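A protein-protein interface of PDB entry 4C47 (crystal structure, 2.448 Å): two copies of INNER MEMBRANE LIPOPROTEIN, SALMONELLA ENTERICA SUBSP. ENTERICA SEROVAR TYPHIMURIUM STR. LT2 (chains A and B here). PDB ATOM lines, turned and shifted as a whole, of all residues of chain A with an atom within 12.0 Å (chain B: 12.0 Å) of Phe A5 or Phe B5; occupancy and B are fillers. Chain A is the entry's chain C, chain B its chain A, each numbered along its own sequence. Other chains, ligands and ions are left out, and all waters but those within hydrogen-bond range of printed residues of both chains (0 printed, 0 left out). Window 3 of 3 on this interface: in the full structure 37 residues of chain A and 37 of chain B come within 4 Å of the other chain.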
ATOM      1  N   ASP A   3     -37.265 -10.967 -31.403  1.00  0.00           N
ATOM      2  CA  ASP A   3     -37.186 -12.090 -32.329  1.00  0.00           C
ATOM      3  C   ASP A   3     -36.141 -11.827 -33.411  1.00  0.00           C
ATOM      4  O   ASP A   3     -35.963 -12.627 -34.329  1.00  0.00           O
ATOM      5  CB  ASP A   3     -38.557 -12.364 -32.961  1.00  0.00           C
ATOM      6  CG  ASP A   3     -38.644 -13.741 -33.600  1.00  0.00           C
ATOM      7  OD1 ASP A   3     -37.815 -14.613 -33.265  1.00  0.00           O
ATOM      8  OD2 ASP A   3     -39.549 -13.954 -34.436  1.00  0.00           O
ATOM      9  N   TYR A   4     -35.454 -10.696 -33.296  1.00  0.00           N
ATOM     10  CA  TYR A   4     -34.367 -10.356 -34.207  1.00  0.00           C
ATOM     11  C   TYR A   4     -33.038 -10.797 -33.618  1.00  0.00           C
ATOM     12  O   TYR A   4     -32.038 -10.914 -34.328  1.00  0.00           O
ATOM     13  CB  TYR A   4     -34.300  -8.845 -34.426  1.00  0.00           C
ATOM     14  CG  TYR A   4     -35.501  -8.233 -35.100  1.00  0.00           C
ATOM     15  CD1 TYR A   4     -36.172  -8.896 -36.119  1.00  0.00           C
ATOM     16  CD2 TYR A   4     -35.960  -6.979 -34.720  1.00  0.00           C
ATOM     17  CE1 TYR A   4     -37.269  -8.327 -36.738  1.00  0.00           C
ATOM     18  CE2 TYR A   4     -37.053  -6.404 -35.329  1.00  0.00           C
ATOM     19  CZ  TYR A   4     -37.704  -7.079 -36.337  1.00  0.00           C
ATOM     20  OH  TYR A   4     -38.796  -6.493 -36.938  1.00  0.00           O
ATOM     21  N   PHE A   5     -33.029 -11.031 -32.310  1.00  0.00           N
ATOM     22  CA  PHE A   5     -31.780 -11.218 -31.588  1.00  0.00           C
ATOM     23  C   PHE A   5     -31.698 -12.565 -30.873  1.00  0.00           C
ATOM     24  O   PHE A   5     -32.692 -13.282 -30.753  1.00  0.00           O
ATOM     25  CB  PHE A   5     -31.576 -10.066 -30.602  1.00  0.00           C
ATOM     26  CG  PHE A   5     -32.005  -8.728 -31.140  1.00  0.00           C
ATOM     27  CD1 PHE A   5     -31.228  -8.060 -32.071  1.00  0.00           C
ATOM     28  CD2 PHE A   5     -33.186  -8.141 -30.715  1.00  0.00           C
ATOM     29  CE1 PHE A   5     -31.621  -6.831 -32.568  1.00  0.00           C
ATOM     30  CE2 PHE A   5     -33.586  -6.910 -31.208  1.00  0.00           C
ATOM     31  CZ  PHE A   5     -32.801  -6.254 -32.136  1.00  0.00           C
ATOM     32  N   ALA A   6     -30.502 -12.897 -30.399  1.00  0.00           N
ATOM     33  CA  ALA A   6     -30.235 -14.211 -29.827  1.00  0.00           C
ATOM     34  C   ALA A   6     -30.276 -14.212 -28.302  1.00  0.00           C
ATOM     35  O   ALA A   6     -29.989 -13.204 -27.659  1.00  0.00           O
ATOM     36  CB  ALA A   6     -28.894 -14.733 -30.318  1.00  0.00           C
ATOM     37  N   ASP A   7     -30.624 -15.362 -27.735  1.00  0.00           N
ATOM     38  CA  ASP A   7     -30.684 -15.529 -26.289  1.00  0.00           C
ATOM     39  C   ASP A   7     -29.282 -15.605 -25.684  1.00  0.00           C
ATOM     40  O   ASP A   7     -28.407 -16.306 -26.199  1.00  0.00           O
ATOM     41  CB  ASP A   7     -31.500 -16.774 -25.928  1.00  0.00           C
ATOM     42  CG  ASP A   7     -31.544 -17.032 -24.435  1.00  0.00           C
ATOM     43  OD1 ASP A   7     -32.287 -16.317 -23.727  1.00  0.00           O
ATOM     44  OD2 ASP A   7     -30.844 -17.958 -23.970  1.00  0.00           O
ATOM     45  N   LYS A   8     -29.082 -14.872 -24.590  1.00  0.00           N
ATOM     46  CA  LYS A   8     -27.782 -14.771 -23.931  1.00  0.00           C
ATOM     47  C   LYS A   8     -27.251 -16.120 -23.437  1.00  0.00           C
ATOM     48  O   LYS A   8     -26.096 -16.475 -23.685  1.00  0.00           O
ATOM     49  CB  LYS A   8     -27.861 -13.761 -22.782  1.00  0.00           C
ATOM     50  CG  LYS A   8     -26.670 -13.771 -21.851  1.00  0.00           C
ATOM     51  CD  LYS A   8     -26.617 -12.520 -20.996  1.00  0.00           C
ATOM     52  CE  LYS A   8     -25.409 -12.529 -20.071  1.00  0.00           C
ATOM     53  NZ  LYS A   8     -25.141 -11.192 -19.474  1.00  0.00           N
ATOM     54  N   HIS A   9     -28.111 -16.865 -22.749  1.00  0.00           N
ATOM     55  CA  HIS A   9     -27.759 -18.169 -22.191  1.00  0.00           C
ATOM     56  C   HIS A   9     -27.313 -19.175 -23.256  1.00  0.00           C
ATOM     57  O   HIS A   9     -26.360 -19.934 -23.048  1.00  0.00           O
ATOM     58  CB  HIS A   9     -28.941 -18.732 -21.392  1.00  0.00           C
ATOM     59  CG  HIS A   9     -28.831 -20.194 -21.090  1.00  0.00           C
ATOM     60  ND1 HIS A   9     -29.762 -21.115 -21.521  1.00  0.00           N
ATOM     61  CD2 HIS A   9     -27.900 -20.895 -20.401  1.00  0.00           C
ATOM     62  CE1 HIS A   9     -29.409 -22.321 -21.109  1.00  0.00           C
ATOM     63  NE2 HIS A   9     -28.283 -22.215 -20.428  1.00  0.00           N
ATOM     64  N   LEU A  10     -28.012 -19.176 -24.387  1.00  0.00           N
ATOM     65  CA  LEU A  10     -27.706 -20.074 -25.498  1.00  0.00           C
ATOM     66  C   LEU A  10     -26.292 -19.802 -26.013  1.00  0.00           C
ATOM     67  O   LEU A  10     -25.498 -20.727 -26.232  1.00  0.00           O
ATOM     68  CB  LEU A  10     -28.743 -19.885 -26.612  1.00  0.00           C
ATOM     69  CG  LEU A  10     -28.834 -20.893 -27.760  1.00  0.00           C
ATOM     70  CD1 LEU A  10     -30.285 -21.265 -28.008  1.00  0.00           C
ATOM     71  CD2 LEU A  10     -28.215 -20.320 -29.020  1.00  0.00           C
ATOM     72  N   VAL A  11     -25.980 -18.520 -26.180  1.00  0.00           N
ATOM     73  CA  VAL A  11     -24.647 -18.092 -26.579  1.00  0.00           C
ATOM     74  C   VAL A  11     -23.604 -18.473 -25.525  1.00  0.00           C
ATOM     75  O   VAL A  11     -22.481 -18.843 -25.865  1.00  0.00           O
ATOM     76  CB  VAL A  11     -24.620 -16.576 -26.890  1.00  0.00           C
ATOM     77  CG1 VAL A  11     -23.199 -16.043 -26.935  1.00  0.00           C
ATOM     78  CG2 VAL A  11     -25.342 -16.304 -28.206  1.00  0.00           C
ATOM     79  N   GLU A  12     -23.985 -18.415 -24.250  1.00  0.00           N
ATOM     80  CA  GLU A  12     -23.090 -18.842 -23.172  1.00  0.00           C
ATOM     81  C   GLU A  12     -22.711 -20.319 -23.340  1.00  0.00           C
ATOM     82  O   GLU A  12     -21.517 -20.683 -23.324  1.00  0.00           O
ATOM     83  CB  GLU A  12     -23.737 -18.602 -21.803  1.00  0.00           C
ATOM     84  CG  GLU A  12     -22.757 -18.256 -20.688  1.00  0.00           C
ATOM     85  CD  GLU A  12     -22.154 -16.869 -20.840  1.00  0.00           C
ATOM     86  OE1 GLU A  12     -22.740 -16.041 -21.570  1.00  0.00           O
ATOM     87  OE2 GLU A  12     -21.091 -16.606 -20.237  1.00  0.00           O
ATOM     88  N   GLU A  13     -23.730 -21.162 -23.513  1.00  0.00           N
ATOM     89  CA  GLU A  13     -23.514 -22.580 -23.790  1.00  0.00           C
ATOM     90  C   GLU A  13     -22.611 -22.773 -25.004  1.00  0.00           C
ATOM     91  O   GLU A  13     -21.715 -23.624 -24.996  1.00  0.00           O
ATOM     92  CB  GLU A  13     -24.846 -23.306 -24.007  1.00  0.00           C
ATOM     93  CG  GLU A  13     -25.645 -23.537 -22.736  1.00  0.00           C
ATOM     94  CD  GLU A  13     -26.400 -24.858 -22.750  1.00  0.00           C
ATOM     95  OE1 GLU A  13     -26.956 -25.216 -23.809  1.00  0.00           O
ATOM     96  OE2 GLU A  13     -26.427 -25.540 -21.702  1.00  0.00           O
ATOM     97  N   MET A  14     -22.850 -21.975 -26.042  1.00  0.00           N
ATOM     98  CA  MET A  14     -22.002 -22.004 -27.229  1.00  0.00           C
ATOM     99  C   MET A  14     -20.542 -21.730 -26.894  1.00  0.00           C
ATOM    100  O   MET A  14     -19.651 -22.400 -27.408  1.00  0.00           O
ATOM    101  CB  MET A  14     -22.471 -20.992 -28.270  1.00  0.00           C
ATOM    102  CG  MET A  14     -23.588 -21.485 -29.156  1.00  0.00           C
ATOM    103  SD  MET A  14     -23.558 -20.638 -30.742  1.00  0.00           S
ATOM    104  CE  MET A  14     -25.304 -20.576 -31.080  1.00  0.00           C
ATOM    105  N   ASP B   3     -28.189  -8.610 -20.052  1.00  0.00           N
ATOM    106  CA  ASP B   3     -29.588  -8.362 -20.376  1.00  0.00           C
ATOM    107  C   ASP B   3     -30.358  -9.667 -20.542  1.00  0.00           C
ATOM    108  O   ASP B   3     -30.199 -10.602 -19.757  1.00  0.00           O
ATOM    109  CB  ASP B   3     -29.700  -7.529 -21.656  1.00  0.00           C
ATOM    110  N   TYR B   4     -31.204  -9.714 -21.566  1.00  0.00           N
ATOM    111  CA  TYR B   4     -31.894 -10.938 -21.948  1.00  0.00           C
ATOM    112  C   TYR B   4     -31.282 -11.465 -23.239  1.00  0.00           C
ATOM    113  O   TYR B   4     -31.518 -12.607 -23.637  1.00  0.00           O
ATOM    114  CB  TYR B   4     -33.388 -10.675 -22.151  1.00  0.00           C
ATOM    115  CG  TYR B   4     -34.183 -10.608 -20.865  1.00  0.00           C
ATOM    116  CD1 TYR B   4     -34.214  -9.449 -20.103  1.00  0.00           C
ATOM    117  CD2 TYR B   4     -34.902 -11.707 -20.417  1.00  0.00           C
ATOM    118  CE1 TYR B   4     -34.937  -9.387 -18.926  1.00  0.00           C
ATOM    119  CE2 TYR B   4     -35.627 -11.658 -19.245  1.00  0.00           C
ATOM    120  CZ  TYR B   4     -35.643 -10.496 -18.502  1.00  0.00           C
ATOM    121  OH  TYR B   4     -36.368 -10.447 -17.332  1.00  0.00           O
ATOM    122  N   PHE B   5     -30.484 -10.620 -23.885  1.00  0.00           N
ATOM    123  CA  PHE B   5     -29.908 -10.947 -25.183  1.00  0.00           C
ATOM    124  C   PHE B   5     -28.386 -11.002 -25.137  1.00  0.00           C
ATOM    125  O   PHE B   5     -27.755 -10.429 -24.248  1.00  0.00           O
ATOM    126  CB  PHE B   5     -30.360  -9.931 -26.234  1.00  0.00           C
ATOM    127  CG  PHE B   5     -31.845  -9.887 -26.434  1.00  0.00           C
ATOM    128  CD1 PHE B   5     -32.457 -10.736 -27.341  1.00  0.00           C
ATOM    129  CD2 PHE B   5     -32.629  -8.998 -25.718  1.00  0.00           C
ATOM    130  CE1 PHE B   5     -33.822 -10.700 -27.532  1.00  0.00           C
ATOM    131  CE2 PHE B   5     -33.993  -8.961 -25.901  1.00  0.00           C
ATOM    132  CZ  PHE B   5     -34.592  -9.812 -26.813  1.00  0.00           C
ATOM    133  N   ALA B   6     -27.802 -11.695 -26.110  1.00  0.00           N
ATOM    134  CA  ALA B   6     -26.355 -11.820 -26.196  1.00  0.00           C
ATOM    135  C   ALA B   6     -25.710 -10.522 -26.661  1.00  0.00           C
ATOM    136  O   ALA B   6     -26.265  -9.795 -27.484  1.00  0.00           O
ATOM    137  CB  ALA B   6     -25.975 -12.960 -27.127  1.00  0.00           C
ATOM    138  N   ASP B   7     -24.530 -10.243 -26.125  1.00  0.00           N
ATOM    139  CA  ASP B   7     -23.765  -9.066 -26.508  1.00  0.00           C
ATOM    140  C   ASP B   7     -23.110  -9.264 -27.879  1.00  0.00           C
ATOM    141  O   ASP B   7     -22.500 -10.299 -28.147  1.00  0.00           O
ATOM    142  CB  ASP B   7     -22.724  -8.760 -25.426  1.00  0.00           C
ATOM    143  CG  ASP B   7     -21.655  -7.787 -25.890  1.00  0.00           C
ATOM    144  OD1 ASP B   7     -21.997  -6.775 -26.535  1.00  0.00           O
ATOM    145  OD2 ASP B   7     -20.464  -8.043 -25.608  1.00  0.00           O
ATOM    146  N   LYS B   8     -23.257  -8.253 -28.732  1.00  0.00           N
ATOM    147  CA  LYS B   8     -22.745  -8.246 -30.102  1.00  0.00           C
ATOM    148  C   LYS B   8     -21.252  -8.574 -30.186  1.00  0.00           C
ATOM    149  O   LYS B   8     -20.840  -9.490 -30.910  1.00  0.00           O
ATOM    150  CB  LYS B   8     -23.011  -6.865 -30.714  1.00  0.00           C
ATOM    151  CG  LYS B   8     -22.742  -6.736 -32.203  1.00  0.00           C
ATOM    152  CD  LYS B   8     -23.852  -7.358 -33.033  1.00  0.00           C
ATOM    153  CE  LYS B   8     -23.817  -6.849 -34.466  1.00  0.00           C
ATOM    154  NZ  LYS B   8     -23.937  -5.364 -34.519  1.00  0.00           N
ATOM    155  N   HIS B   9     -20.453  -7.819 -29.434  1.00  0.00           N
ATOM    156  CA  HIS B   9     -18.998  -7.955 -29.430  1.00  0.00           C
ATOM    157  C   HIS B   9     -18.537  -9.360 -29.063  1.00  0.00           C
ATOM    158  O   HIS B   9     -17.648  -9.922 -29.703  1.00  0.00           O
ATOM    159  CB  HIS B   9     -18.380  -6.945 -28.459  1.00  0.00           C
ATOM    160  CG  HIS B   9     -16.901  -7.102 -28.281  1.00  0.00           C
ATOM    161  ND1 HIS B   9     -16.342  -7.681 -27.161  1.00  0.00           N
ATOM    162  CD2 HIS B   9     -15.866  -6.751 -29.080  1.00  0.00           C
ATOM    163  CE1 HIS B   9     -15.027  -7.681 -27.280  1.00  0.00           C
ATOM    164  NE2 HIS B   9     -14.712  -7.123 -28.434  1.00  0.00           N
ATOM    165  N   LEU B  10     -19.145  -9.911 -28.017  1.00  0.00           N
ATOM    166  CA  LEU B  10     -18.845 -11.258 -27.553  1.00  0.00           C
ATOM    167  C   LEU B  10     -19.104 -12.270 -28.672  1.00  0.00           C
ATOM    168  O   LEU B  10     -18.305 -13.184 -28.902  1.00  0.00           O
ATOM    169  CB  LEU B  10     -19.697 -11.571 -26.320  1.00  0.00           C
ATOM    170  CG  LEU B  10     -19.244 -12.665 -25.349  1.00  0.00           C
ATOM    171  CD1 LEU B  10     -19.707 -14.037 -25.810  1.00  0.00           C
ATOM    172  CD2 LEU B  10     -17.731 -12.637 -25.173  1.00  0.00           C
ATOM    173  N   VAL B  11     -20.220 -12.088 -29.372  1.00  0.00           N
ATOM    174  CA  VAL B  11     -20.572 -12.944 -30.502  1.00  0.00           C
ATOM    175  C   VAL B  11     -19.559 -12.829 -31.640  1.00  0.00           C
ATOM    176  O   VAL B  11     -19.204 -13.831 -32.262  1.00  0.00           O
ATOM    177  CB  VAL B  11     -22.013 -12.670 -31.004  1.00  0.00           C
ATOM    178  CG1 VAL B  11     -22.133 -12.916 -32.504  1.00  0.00           C
ATOM    179  CG2 VAL B  11     -23.004 -13.531 -30.235  1.00  0.00           C
ATOM    180  N   GLU B  12     -19.085 -11.614 -31.899  1.00  0.00           N
ATOM    181  CA  GLU B  12     -18.045 -11.413 -32.903  1.00  0.00           C
ATOM    182  C   GLU B  12     -16.760 -12.149 -32.520  1.00  0.00           C
ATOM    183  O   GLU B  12     -16.148 -12.822 -33.357  1.00  0.00           O
ATOM    184  CB  GLU B  12     -17.771  -9.922 -33.117  1.00  0.00           C
ATOM    185  CG  GLU B  12     -18.700  -9.257 -34.122  1.00  0.00           C
ATOM    186  CD  GLU B  12     -18.472  -9.749 -35.541  1.00  0.00           C
ATOM    187  OE1 GLU B  12     -17.309 -10.041 -35.895  1.00  0.00           O
ATOM    188  OE2 GLU B  12     -19.458  -9.846 -36.301  1.00  0.00           O
ATOM    189  N   MET B  14     -16.483 -14.785 -30.542  1.00  0.00           N
ATOM    190  CA  MET B  14     -16.768 -16.207 -30.721  1.00  0.00           C
ATOM    191  C   MET B  14     -16.706 -16.639 -32.186  1.00  0.00           C
ATOM    192  O   MET B  14     -16.144 -17.686 -32.500  1.00  0.00           O
ATOM    193  CB  MET B  14     -18.132 -16.569 -30.135  1.00  0.00           C
ATOM    194  CG  MET B  14     -18.121 -16.782 -28.632  1.00  0.00           C
ATOM    195  SD  MET B  14     -19.777 -17.085 -27.994  1.00  0.00           S
ATOM    196  CE  MET B  14     -20.399 -18.225 -29.226  1.00  0.00           C
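The side-chain carboxylate (OD2) of Asp A7 is in hydrogen-bond range of the backbone NH (N) of Leu A10 (3.1 Å). The side-chain carboxylate (OD2) of Asp A7 lies within hydrogen-bond range of the backbone NH (N) of His A9.
No residue of chain B comes within 4 Å of Tyr A4. Printed residues of chain B within 4 Å of Phe A5: Phe B5 (3.4 Å). Of chain B, only Tyr B4 (3.5 Å), Phe B5 (3.6 Å) and Ala B6 (3.7 Å) come within 4 Å of Lys A8. Of the printed residues of chain B, Val A11 touches Ala B6 and Met B14. Of the printed residues of chain B, Met A14 touches Met B14. No residue of chain A comes within 4 Å of Asp B3. Printed residues of chain A within 4 Å of Tyr B4: Asp A7 (3.8 Å) and Lys A8 (3.5 Å). Phe B5 touches three residues of chain A. Printed residues of chain A within 4 Å of Ala B6: Ala A6, Lys A8 and Val A11. No residue of chain A comes within 4 Å of Asp B7. The nearest residue of chain A that does not touch Phe B5 is Asp A7 (4.7 Å).
Of the 11 printed residues of chain B, 4 touch a printed residue of chain A. Printed residues of chain B that touch a printed residue of chain A: Tyr B4, Phe B5, Ala B6 and Met B14. Along chain B the printed residues that touch a printed residue of chain A span positions 4 to 14. Of the 12 printed residues of chain A, 6 touch a printed residue of chain B. Hydrophobic or aromatic side chains of chain A within 4 Å of the printed part of chain B: Phe A5, Val A11 and Met A14. Among the printed residues, 10 pairs touch across the chains. Among the printed residues, no Asp or Glu carboxylate lies within 4 Å of a Lys or Arg side-chain nitrogen of the other chain.
Among the printed residues, pairs that only touch across the chains: Ala A6 with Phe B5 (3.4 Å), Phe A5 with Phe B5 (3.4 Å), Val A11 with Ala B6 (3.6 Å), Met A14 with Met B14 (3.6 Å), Lys A8 with Phe B5 (3.6 Å), Val A11 with Met B14 (3.7 Å), Lys A8 with Ala B6 (3.7 Å) and Asp A7 with Tyr B4 (3.8 Å).
Phe B5 touches its own counterpart, Phe A5. Asp A7 touches Tyr B4, but with the chains exchanged Tyr A4 does not touch Asp B7 (11.1 Å). Val A11 touches Ala B6, but with the chains exchanged Ala A6 does not touch Val B11 (6.0 Å). Val A11 touches Met B14, but with the chains exchanged Met A14 does not touch Val B11 (7.1 Å). Positions printed for both chains: 3, 4, 5, 6, 7, 8, 9, 10, 11, 12 and 14. Of the 10 pairs that touch across the chains among the printed residues, 3 have their exchanged pair printed and touching as well.
N of Ala B6 sits at hydrogen-bond distance from O of Ala A6 (3.1 Å). The backbone NH of Lys A8 is in hydrogen-bond range of the backbone carbonyl oxygen of Tyr B4, at 3.5 Å.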
